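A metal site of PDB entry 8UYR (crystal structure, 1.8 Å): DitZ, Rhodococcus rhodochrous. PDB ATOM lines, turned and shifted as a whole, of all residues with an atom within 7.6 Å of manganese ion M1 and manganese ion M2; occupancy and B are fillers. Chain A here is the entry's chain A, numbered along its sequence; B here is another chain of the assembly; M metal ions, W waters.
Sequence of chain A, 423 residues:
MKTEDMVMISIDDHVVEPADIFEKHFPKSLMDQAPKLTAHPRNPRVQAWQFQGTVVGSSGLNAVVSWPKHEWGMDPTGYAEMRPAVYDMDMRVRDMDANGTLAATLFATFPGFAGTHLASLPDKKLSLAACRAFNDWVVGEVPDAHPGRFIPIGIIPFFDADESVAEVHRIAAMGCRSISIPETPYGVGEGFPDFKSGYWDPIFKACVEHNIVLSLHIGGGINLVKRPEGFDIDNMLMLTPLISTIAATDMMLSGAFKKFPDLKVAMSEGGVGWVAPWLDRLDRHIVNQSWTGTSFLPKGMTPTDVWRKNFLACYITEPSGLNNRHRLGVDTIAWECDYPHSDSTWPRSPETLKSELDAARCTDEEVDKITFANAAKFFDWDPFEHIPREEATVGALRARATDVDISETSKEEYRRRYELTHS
Manganese ion M1 is bound by the side-chain carboxylate (OD1) of Asp 338, the side-chain carboxylate (OE1) of Glu 269, a ring nitrogen (NE2) of His 217, a ring nitrogen (NE2) of His 14, the side-chain carboxylate (OD2) of Asp 12 and the side-chain carboxylate (OD1) of Asp 12.
Three residues have an atom within 4 Å of manganese ion M2: Glu 269, Asp 338 and His 341.
The nearest printed residue that does not touch manganese ion M2 is His 14 (4.2 Å).
OD2 of Asp 13 is in hydrogen-bond range of N of Asp 338, 3.3 Å away.
The side-chain carboxylate (OE2) of Glu 336 lies within hydrogen-bond range of the backbone NH (N) of Glu 269 (2.8 Å).
A ring nitrogen (NE2) of His 341 lies close to a ring nitrogen (ND1) of His 14.
A ring nitrogen (NE2) of His 341 sits at hydrogen-bond distance from the side-chain amide oxygen of Asn 62, at 3.5 Å.
The backbone NH (N) of His 14 sits at hydrogen-bond distance from the backbone carbonyl oxygen (O) of Tyr 339, 2.8 Å away.
OD2 of Asp 12 sits close to OE1 of Glu 336 (2.5 Å).
Within 4 Å of manganese ion M1: Asp 12, His 14, His 217, Glu 269 and Asp 338.
Water W1 binds manganese ion M2, 2.1 Å away.
OD2 of Asp 338 binds manganese ion M2 (2.1 Å).
Water W2 binds manganese ion M2, 2.2 Å away.
Manganese ion M2 is bound by ND1 of His 341 (2.2 Å).
OE2 of Glu 269 is bound to manganese ion M2 (2.2 Å).
Manganese ion M2 is bound by the side-chain carboxylate (OE1) of Glu 269, at 2.4 Å.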
ATOM      1  N   ILE A  11     -10.102 -19.486  21.193  1.00  0.00           N
ATOM      2  CA  ILE A  11     -11.123 -20.054  20.295  1.00  0.00           C
ATOM      3  C   ILE A  11     -12.536 -19.688  20.760  1.00  0.00           C
ATOM      4  O   ILE A  11     -13.507 -20.325  20.360  1.00  0.00           O
ATOM      5  CB  ILE A  11     -10.961 -21.574  20.101  1.00  0.00           C
ATOM      6  CG1 ILE A  11     -10.527 -22.265  21.382  1.00  0.00           C
ATOM      7  CG2 ILE A  11      -9.987 -21.882  18.927  1.00  0.00           C
ATOM      8  CD1 ILE A  11     -11.609 -22.325  22.397  1.00  0.00           C
ATOM      9  N   ASP A  12     -12.683 -18.629  21.567  1.00  0.00           N
ATOM     10  CA  ASP A  12     -14.007 -18.131  21.908  1.00  0.00           C
ATOM     11  C   ASP A  12     -13.852 -16.676  22.334  1.00  0.00           C
ATOM     12  O   ASP A  12     -13.348 -16.406  23.429  1.00  0.00           O
ATOM     13  CB  ASP A  12     -14.635 -18.987  23.010  1.00  0.00           C
ATOM     14  CG  ASP A  12     -15.890 -18.358  23.601  1.00  0.00           C
ATOM     15  OD1 ASP A  12     -16.525 -17.520  22.926  1.00  0.00           O
ATOM     16  OD2 ASP A  12     -16.259 -18.734  24.737  1.00  0.00           O
ATOM     17  N   ASP A  13     -14.282 -15.761  21.471  1.00  0.00           N
ATOM     18  CA  ASP A  13     -14.486 -14.360  21.821  1.00  0.00           C
ATOM     19  C   ASP A  13     -15.801 -13.927  21.223  1.00  0.00           C
ATOM     20  O   ASP A  13     -16.490 -14.709  20.555  1.00  0.00           O
ATOM     21  CB  ASP A  13     -13.319 -13.511  21.335  1.00  0.00           C
ATOM     22  CG  ASP A  13     -11.996 -13.991  21.872  1.00  0.00           C
ATOM     23  OD1 ASP A  13     -11.422 -14.915  21.259  1.00  0.00           O
ATOM     24  OD2 ASP A  13     -11.559 -13.490  22.930  1.00  0.00           O
ATOM     25  N   HIS A  14     -16.158 -12.670  21.429  1.00  0.00           N
ATOM     26  CA  HIS A  14     -17.432 -12.147  20.974  1.00  0.00           C
ATOM     27  C   HIS A  14     -17.221 -10.813  20.283  1.00  0.00           C
ATOM     28  O   HIS A  14     -16.283 -10.076  20.603  1.00  0.00           O
ATOM     29  CB  HIS A  14     -18.399 -12.051  22.153  1.00  0.00           C
ATOM     30  CG  HIS A  14     -18.723 -13.376  22.768  1.00  0.00           C
ATOM     31  ND1 HIS A  14     -19.829 -14.104  22.406  1.00  0.00           N
ATOM     32  CD2 HIS A  14     -18.069 -14.115  23.690  1.00  0.00           C
ATOM     33  CE1 HIS A  14     -19.853 -15.238  23.090  1.00  0.00           C
ATOM     34  NE2 HIS A  14     -18.789 -15.267  23.877  1.00  0.00           N
ATOM     35  N   LEU A  61     -23.436  -7.440  30.402  1.00  0.00           N
ATOM     36  CA  LEU A  61     -22.396  -8.343  30.896  1.00  0.00           C
ATOM     37  C   LEU A  61     -21.484  -8.812  29.775  1.00  0.00           C
ATOM     38  O   LEU A  61     -20.513  -9.535  30.037  1.00  0.00           O
ATOM     39  CB  LEU A  61     -22.994  -9.560  31.600  1.00  0.00           C
ATOM     40  CG  LEU A  61     -23.802  -9.327  32.868  1.00  0.00           C
ATOM     41  CD1 LEU A  61     -24.377 -10.657  33.351  1.00  0.00           C
ATOM     42  CD2 LEU A  61     -22.969  -8.650  33.954  1.00  0.00           C
ATOM     43  N   ASN A  62     -21.779  -8.441  28.540  1.00  0.00           N
ATOM     44  CA  ASN A  62     -21.099  -9.007  27.385  1.00  0.00           C
ATOM     45  C   ASN A  62     -20.150  -8.037  26.706  1.00  0.00           C
ATOM     46  O   ASN A  62     -19.524  -8.395  25.712  1.00  0.00           O
ATOM     47  CB  ASN A  62     -22.140  -9.525  26.390  1.00  0.00           C
ATOM     48  CG  ASN A  62     -22.830 -10.785  26.885  1.00  0.00           C
ATOM     49  OD1 ASN A  62     -22.375 -11.413  27.836  1.00  0.00           O
ATOM     50  ND2 ASN A  62     -23.937 -11.151  26.233  1.00  0.00           N
ATOM     51  N   THR A 105     -11.597 -15.678  18.022  1.00  0.00           N
ATOM     52  CA  THR A 105     -12.636 -16.406  17.303  1.00  0.00           C
ATOM     53  C   THR A 105     -13.970 -15.731  17.620  1.00  0.00           C
ATOM     54  O   THR A 105     -14.477 -15.868  18.738  1.00  0.00           O
ATOM     55  CB  THR A 105     -12.648 -17.879  17.717  1.00  0.00           C
ATOM     56  OG1 THR A 105     -11.338 -18.438  17.534  1.00  0.00           O
ATOM     57  CG2 THR A 105     -13.623 -18.689  16.909  1.00  0.00           C
ATOM     58  N   PHE A 107     -17.628 -14.823  17.995  1.00  0.00           N
ATOM     59  CA  PHE A 107     -19.037 -15.194  18.032  1.00  0.00           C
ATOM     60  C   PHE A 107     -19.938 -13.961  17.898  1.00  0.00           C
ATOM     61  O   PHE A 107     -19.646 -12.906  18.474  1.00  0.00           O
ATOM     62  CB  PHE A 107     -19.374 -15.943  19.325  1.00  0.00           C
ATOM     63  CG  PHE A 107     -18.917 -17.384  19.351  1.00  0.00           C
ATOM     64  CD1 PHE A 107     -17.628 -17.719  19.717  1.00  0.00           C
ATOM     65  CD2 PHE A 107     -19.777 -18.408  18.994  1.00  0.00           C
ATOM     66  CE1 PHE A 107     -17.206 -19.033  19.722  1.00  0.00           C
ATOM     67  CE2 PHE A 107     -19.367 -19.712  19.007  1.00  0.00           C
ATOM     68  CZ  PHE A 107     -18.085 -20.035  19.374  1.00  0.00           C
ATOM     69  N   PHE A 113     -25.288 -15.668  19.076  1.00  0.00           N
ATOM     70  CA  PHE A 113     -23.999 -16.311  18.791  1.00  0.00           C
ATOM     71  C   PHE A 113     -24.174 -17.619  18.026  1.00  0.00           C
ATOM     72  O   PHE A 113     -23.224 -18.107  17.419  1.00  0.00           O
ATOM     73  CB  PHE A 113     -23.220 -16.561  20.077  1.00  0.00           C
ATOM     74  CG  PHE A 113     -24.009 -17.245  21.149  1.00  0.00           C
ATOM     75  CD1 PHE A 113     -24.238 -18.610  21.106  1.00  0.00           C
ATOM     76  CD2 PHE A 113     -24.533 -16.510  22.203  1.00  0.00           C
ATOM     77  CE1 PHE A 113     -24.992 -19.243  22.082  1.00  0.00           C
ATOM     78  CE2 PHE A 113     -25.280 -17.138  23.194  1.00  0.00           C
ATOM     79  CZ  PHE A 113     -25.504 -18.509  23.129  1.00  0.00           C
ATOM     80  N   HIS A 217     -21.534 -23.314  21.767  1.00  0.00           N
ATOM     81  CA  HIS A 217     -21.278 -22.325  22.808  1.00  0.00           C
ATOM     82  C   HIS A 217     -22.337 -22.391  23.907  1.00  0.00           C
ATOM     83  O   HIS A 217     -23.527 -22.632  23.630  1.00  0.00           O
ATOM     84  CB  HIS A 217     -21.254 -20.937  22.196  1.00  0.00           C
ATOM     85  CG  HIS A 217     -20.675 -19.879  23.082  1.00  0.00           C
ATOM     86  ND1 HIS A 217     -21.357 -19.342  24.154  1.00  0.00           N
ATOM     87  CD2 HIS A 217     -19.490 -19.214  23.037  1.00  0.00           C
ATOM     88  CE1 HIS A 217     -20.614 -18.422  24.740  1.00  0.00           C
ATOM     89  NE2 HIS A 217     -19.471 -18.331  24.083  1.00  0.00           N
ATOM     90  N   ILE A 218     -21.917 -22.191  25.162  1.00  0.00           N
ATOM     91  CA  ILE A 218     -22.866 -22.178  26.288  1.00  0.00           C
ATOM     92  C   ILE A 218     -23.934 -21.095  26.080  1.00  0.00           C
ATOM     93  O   ILE A 218     -23.746 -20.112  25.343  1.00  0.00           O
ATOM     94  CB  ILE A 218     -22.149 -21.947  27.623  1.00  0.00           C
ATOM     95  CG1 ILE A 218     -21.621 -20.511  27.678  1.00  0.00           C
ATOM     96  CG2 ILE A 218     -21.022 -22.952  27.814  1.00  0.00           C
ATOM     97  CD1 ILE A 218     -20.989 -20.140  29.018  1.00  0.00           C
ATOM     98  N   PRO A 241     -22.295 -21.665  32.792  1.00  0.00           N
ATOM     99  CA  PRO A 241     -21.140 -22.302  32.138  1.00  0.00           C
ATOM    100  C   PRO A 241     -20.757 -23.663  32.698  1.00  0.00           C
ATOM    101  O   PRO A 241     -19.728 -24.200  32.265  1.00  0.00           O
ATOM    102  CB  PRO A 241     -20.028 -21.292  32.384  1.00  0.00           C
ATOM    103  CG  PRO A 241     -20.356 -20.737  33.742  1.00  0.00           C
ATOM    104  CD  PRO A 241     -21.852 -20.694  33.815  1.00  0.00           C
ATOM    105  N   SER A 268     -17.550 -24.692  23.288  1.00  0.00           N
ATOM    106  CA  SER A 268     -17.061 -23.338  23.519  1.00  0.00           C
ATOM    107  C   SER A 268     -17.558 -22.766  24.846  1.00  0.00           C
ATOM    108  O   SER A 268     -18.755 -22.816  25.151  1.00  0.00           O
ATOM    109  CB  SER A 268     -17.483 -22.450  22.358  1.00  0.00           C
ATOM    110  OG  SER A 268     -17.243 -23.129  21.127  1.00  0.00           O
ATOM    111  N   GLU A 269     -16.633 -22.223  25.625  1.00  0.00           N
ATOM    112  CA  GLU A 269     -16.896 -21.629  26.951  1.00  0.00           C
ATOM    113  C   GLU A 269     -17.444 -22.641  27.955  1.00  0.00           C
ATOM    114  O   GLU A 269     -18.003 -22.263  28.990  1.00  0.00           O
ATOM    115  CB  GLU A 269     -17.838 -20.411  26.864  1.00  0.00           C
ATOM    116  CG  GLU A 269     -17.480 -19.339  27.961  1.00  0.00           C
ATOM    117  CD  GLU A 269     -18.258 -18.026  27.881  1.00  0.00           C
ATOM    118  OE1 GLU A 269     -18.551 -17.521  26.772  1.00  0.00           O
ATOM    119  OE2 GLU A 269     -18.566 -17.464  28.964  1.00  0.00           O
ATOM    120  N   GLY A 270     -17.253 -23.929  27.699  1.00  0.00           N
ATOM    121  CA  GLY A 270     -17.784 -24.918  28.606  1.00  0.00           C
ATOM    122  C   GLY A 270     -16.941 -25.249  29.803  1.00  0.00           C
ATOM    123  O   GLY A 270     -17.430 -25.893  30.728  1.00  0.00           O
ATOM    124  N   ILE A 316     -11.457 -20.535  29.973  1.00  0.00           N
ATOM    125  CA  ILE A 316     -10.804 -19.254  30.211  1.00  0.00           C
ATOM    126  C   ILE A 316      -9.853 -19.377  31.382  1.00  0.00           C
ATOM    127  O   ILE A 316      -8.647 -19.102  31.290  1.00  0.00           O
ATOM    128  CB  ILE A 316     -11.846 -18.163  30.507  1.00  0.00           C
ATOM    129  CG1 ILE A 316     -12.948 -18.147  29.441  1.00  0.00           C
ATOM    130  CG2 ILE A 316     -11.175 -16.801  30.627  1.00  0.00           C
ATOM    131  CD1 ILE A 316     -14.198 -17.403  29.914  1.00  0.00           C
ATOM    132  N   GLU A 336      -9.266 -19.974  25.887  1.00  0.00           N
ATOM    133  CA  GLU A 336     -10.025 -18.912  25.240  1.00  0.00           C
ATOM    134  C   GLU A 336     -10.001 -17.683  26.127  1.00  0.00           C
ATOM    135  O   GLU A 336      -9.879 -17.789  27.346  1.00  0.00           O
ATOM    136  CB  GLU A 336     -11.470 -19.321  24.971  1.00  0.00           C
ATOM    137  CG  GLU A 336     -12.111 -19.939  26.170  1.00  0.00           C
ATOM    138  CD  GLU A 336     -13.599 -20.079  25.981  1.00  0.00           C
ATOM    139  OE1 GLU A 336     -14.316 -19.110  26.283  1.00  0.00           O
ATOM    140  OE2 GLU A 336     -14.026 -21.131  25.483  1.00  0.00           O
ATOM    141  N   CYS A 337     -10.169 -16.509  25.495  1.00  0.00           N
ATOM    142  CA  CYS A 337     -10.147 -15.248  26.224  1.00  0.00           C
ATOM    143  C   CYS A 337     -11.544 -14.760  26.610  1.00  0.00           C
ATOM    144  O   CYS A 337     -11.703 -14.155  27.673  1.00  0.00           O
ATOM    145  CB  CYS A 337      -9.470 -14.173  25.370  1.00  0.00           C
ATOM    146  SG  CYS A 337      -9.153 -12.619  26.262  1.00  0.00           S
ATOM    147  N   ASP A 338     -12.529 -14.994  25.737  1.00  0.00           N
ATOM    148  CA  ASP A 338     -13.927 -14.575  25.913  1.00  0.00           C
ATOM    149  C   ASP A 338     -14.066 -13.055  25.973  1.00  0.00           C
ATOM    150  O   ASP A 338     -14.990 -12.535  26.596  1.00  0.00           O
ATOM    151  CB  ASP A 338     -14.571 -15.227  27.126  1.00  0.00           C
ATOM    152  CG  ASP A 338     -16.085 -15.408  26.950  1.00  0.00           C
ATOM    153  OD1 ASP A 338     -16.520 -15.687  25.805  1.00  0.00           O
ATOM    154  OD2 ASP A 338     -16.814 -15.247  27.963  1.00  0.00           O
ATOM    155  N   TYR A 339     -13.157 -12.351  25.334  1.00  0.00           N
ATOM    156  CA  TYR A 339     -13.269 -10.908  25.193  1.00  0.00           C
ATOM    157  C   TYR A 339     -14.535 -10.571  24.410  1.00  0.00           C
ATOM    158  O   TYR A 339     -14.836 -11.226  23.407  1.00  0.00           O
ATOM    159  CB  TYR A 339     -12.022 -10.396  24.464  1.00  0.00           C
ATOM    160  CG  TYR A 339     -11.922  -8.906  24.285  1.00  0.00           C
ATOM    161  CD1 TYR A 339     -12.762  -8.231  23.409  1.00  0.00           C
ATOM    162  CD2 TYR A 339     -10.943  -8.167  24.961  1.00  0.00           C
ATOM    163  CE1 TYR A 339     -12.671  -6.864  23.224  1.00  0.00           C
ATOM    164  CE2 TYR A 339     -10.850  -6.790  24.778  1.00  0.00           C
ATOM    165  CZ  TYR A 339     -11.713  -6.154  23.907  1.00  0.00           C
ATOM    166  OH  TYR A 339     -11.626  -4.791  23.697  1.00  0.00           O
ATOM    167  N   PRO A 340     -15.317  -9.561  24.837  1.00  0.00           N
ATOM    168  CA  PRO A 340     -15.199  -8.662  25.991  1.00  0.00           C
ATOM    169  C   PRO A 340     -16.184  -8.998  27.109  1.00  0.00           C
ATOM    170  O   PRO A 340     -16.675  -8.094  27.783  1.00  0.00           O
ATOM    171  CB  PRO A 340     -15.538  -7.293  25.373  1.00  0.00           C
ATOM    172  CG  PRO A 340     -16.465  -7.616  24.167  1.00  0.00           C
ATOM    173  CD  PRO A 340     -16.416  -9.141  23.950  1.00  0.00           C
ATOM    174  N   HIS A 341     -16.462 -10.282  27.303  1.00  0.00           N
ATOM    175  CA  HIS A 341     -17.429 -10.722  28.288  1.00  0.00           C
ATOM    176  C   HIS A 341     -16.911 -10.519  29.703  1.00  0.00           C
ATOM    177  O   HIS A 341     -15.703 -10.451  29.953  1.00  0.00           O
ATOM    178  CB  HIS A 341     -17.755 -12.204  28.117  1.00  0.00           C
ATOM    179  CG  HIS A 341     -18.783 -12.475  27.056  1.00  0.00           C
ATOM    180  ND1 HIS A 341     -19.432 -13.688  26.953  1.00  0.00           N
ATOM    181  CD2 HIS A 341     -19.261 -11.704  26.058  1.00  0.00           C
ATOM    182  CE1 HIS A 341     -20.270 -13.646  25.931  1.00  0.00           C
ATOM    183  NE2 HIS A 341     -20.186 -12.460  25.368  1.00  0.00           N
ATOM    184  N   SER A 342     -17.865 -10.477  30.646  1.00  0.00           N
ATOM    185  CA  SER A 342     -17.560 -10.408  32.070  1.00  0.00           C
ATOM    186  C   SER A 342     -16.574 -11.488  32.519  1.00  0.00           C
ATOM    187  O   SER A 342     -15.796 -11.255  33.452  1.00  0.00           O
ATOM    188  CB  SER A 342     -18.862 -10.516  32.857  1.00  0.00           C
ATOM    189  OG  SER A 342     -19.647 -11.615  32.417  1.00  0.00           O
ATOM    190  N   ASP A 343     -16.592 -12.650  31.888  1.00  0.00           N
ATOM    191  CA  ASP A 343     -15.699 -13.732  32.289  1.00  0.00           C
ATOM    192  C   ASP A 343     -14.297 -13.626  31.716  1.00  0.00           C
ATOM    193  O   ASP A 343     -13.414 -14.379  32.146  1.00  0.00           O
ATOM    194  CB  ASP A 343     -16.318 -15.083  31.897  1.00  0.00           C
ATOM    195  CG  ASP A 343     -17.491 -15.473  32.789  1.00  0.00           C
ATOM    196  OD1 ASP A 343     -17.242 -15.751  33.980  1.00  0.00           O
ATOM    197  OD2 ASP A 343     -18.647 -15.478  32.310  1.00  0.00           O
ATOM    198  N   SER A 344     -14.038 -12.699  30.789  1.00  0.00           N
ATOM    199  CA  SER A 344     -12.715 -12.584  30.197  1.00  0.00           C
ATOM    200  C   SER A 344     -11.631 -12.254  31.237  1.00  0.00           C
ATOM    201  O   SER A 344     -11.877 -11.550  32.220  1.00  0.00           O
ATOM    202  CB  SER A 344     -12.704 -11.511  29.124  1.00  0.00           C
ATOM    203  OG  SER A 344     -11.428 -11.427  28.519  1.00  0.00           O
ATOM    204  N   ARG B 281     -15.319 -21.755  40.177  1.00  0.00           N
ATOM    205  CA  ARG B 281     -16.163 -20.635  39.759  1.00  0.00           C
ATOM    206  C   ARG B 281     -16.729 -19.878  40.953  1.00  0.00           C
ATOM    207  O   ARG B 281     -16.806 -18.650  40.926  1.00  0.00           O
ATOM    208  CB  ARG B 281     -17.280 -21.130  38.848  1.00  0.00           C
ATOM    209  CG  ARG B 281     -18.031 -19.960  38.225  1.00  0.00           C
ATOM    210  CD  ARG B 281     -18.927 -20.378  37.078  1.00  0.00           C
ATOM    211  NE  ARG B 281     -19.610 -19.203  36.549  1.00  0.00           N
ATOM    212  CZ  ARG B 281     -19.043 -18.312  35.747  1.00  0.00           C
ATOM    213  NH1 ARG B 281     -17.769 -18.469  35.344  1.00  0.00           N
ATOM    214  NH2 ARG B 281     -19.743 -17.268  35.327  1.00  0.00           N
HETATM  215 MN    MN M   1     -17.841 -17.059  24.771  1.00  0.00          MN
HETATM  216 MN    MN M   2     -18.923 -15.485  28.077  1.00  0.00          MN
HETATM  217  O   HOH W   1     -20.941 -16.130  27.929  1.00  0.00           O
HETATM  218  O   HOH W   2     -19.132 -14.526  30.010  1.00  0.00           O
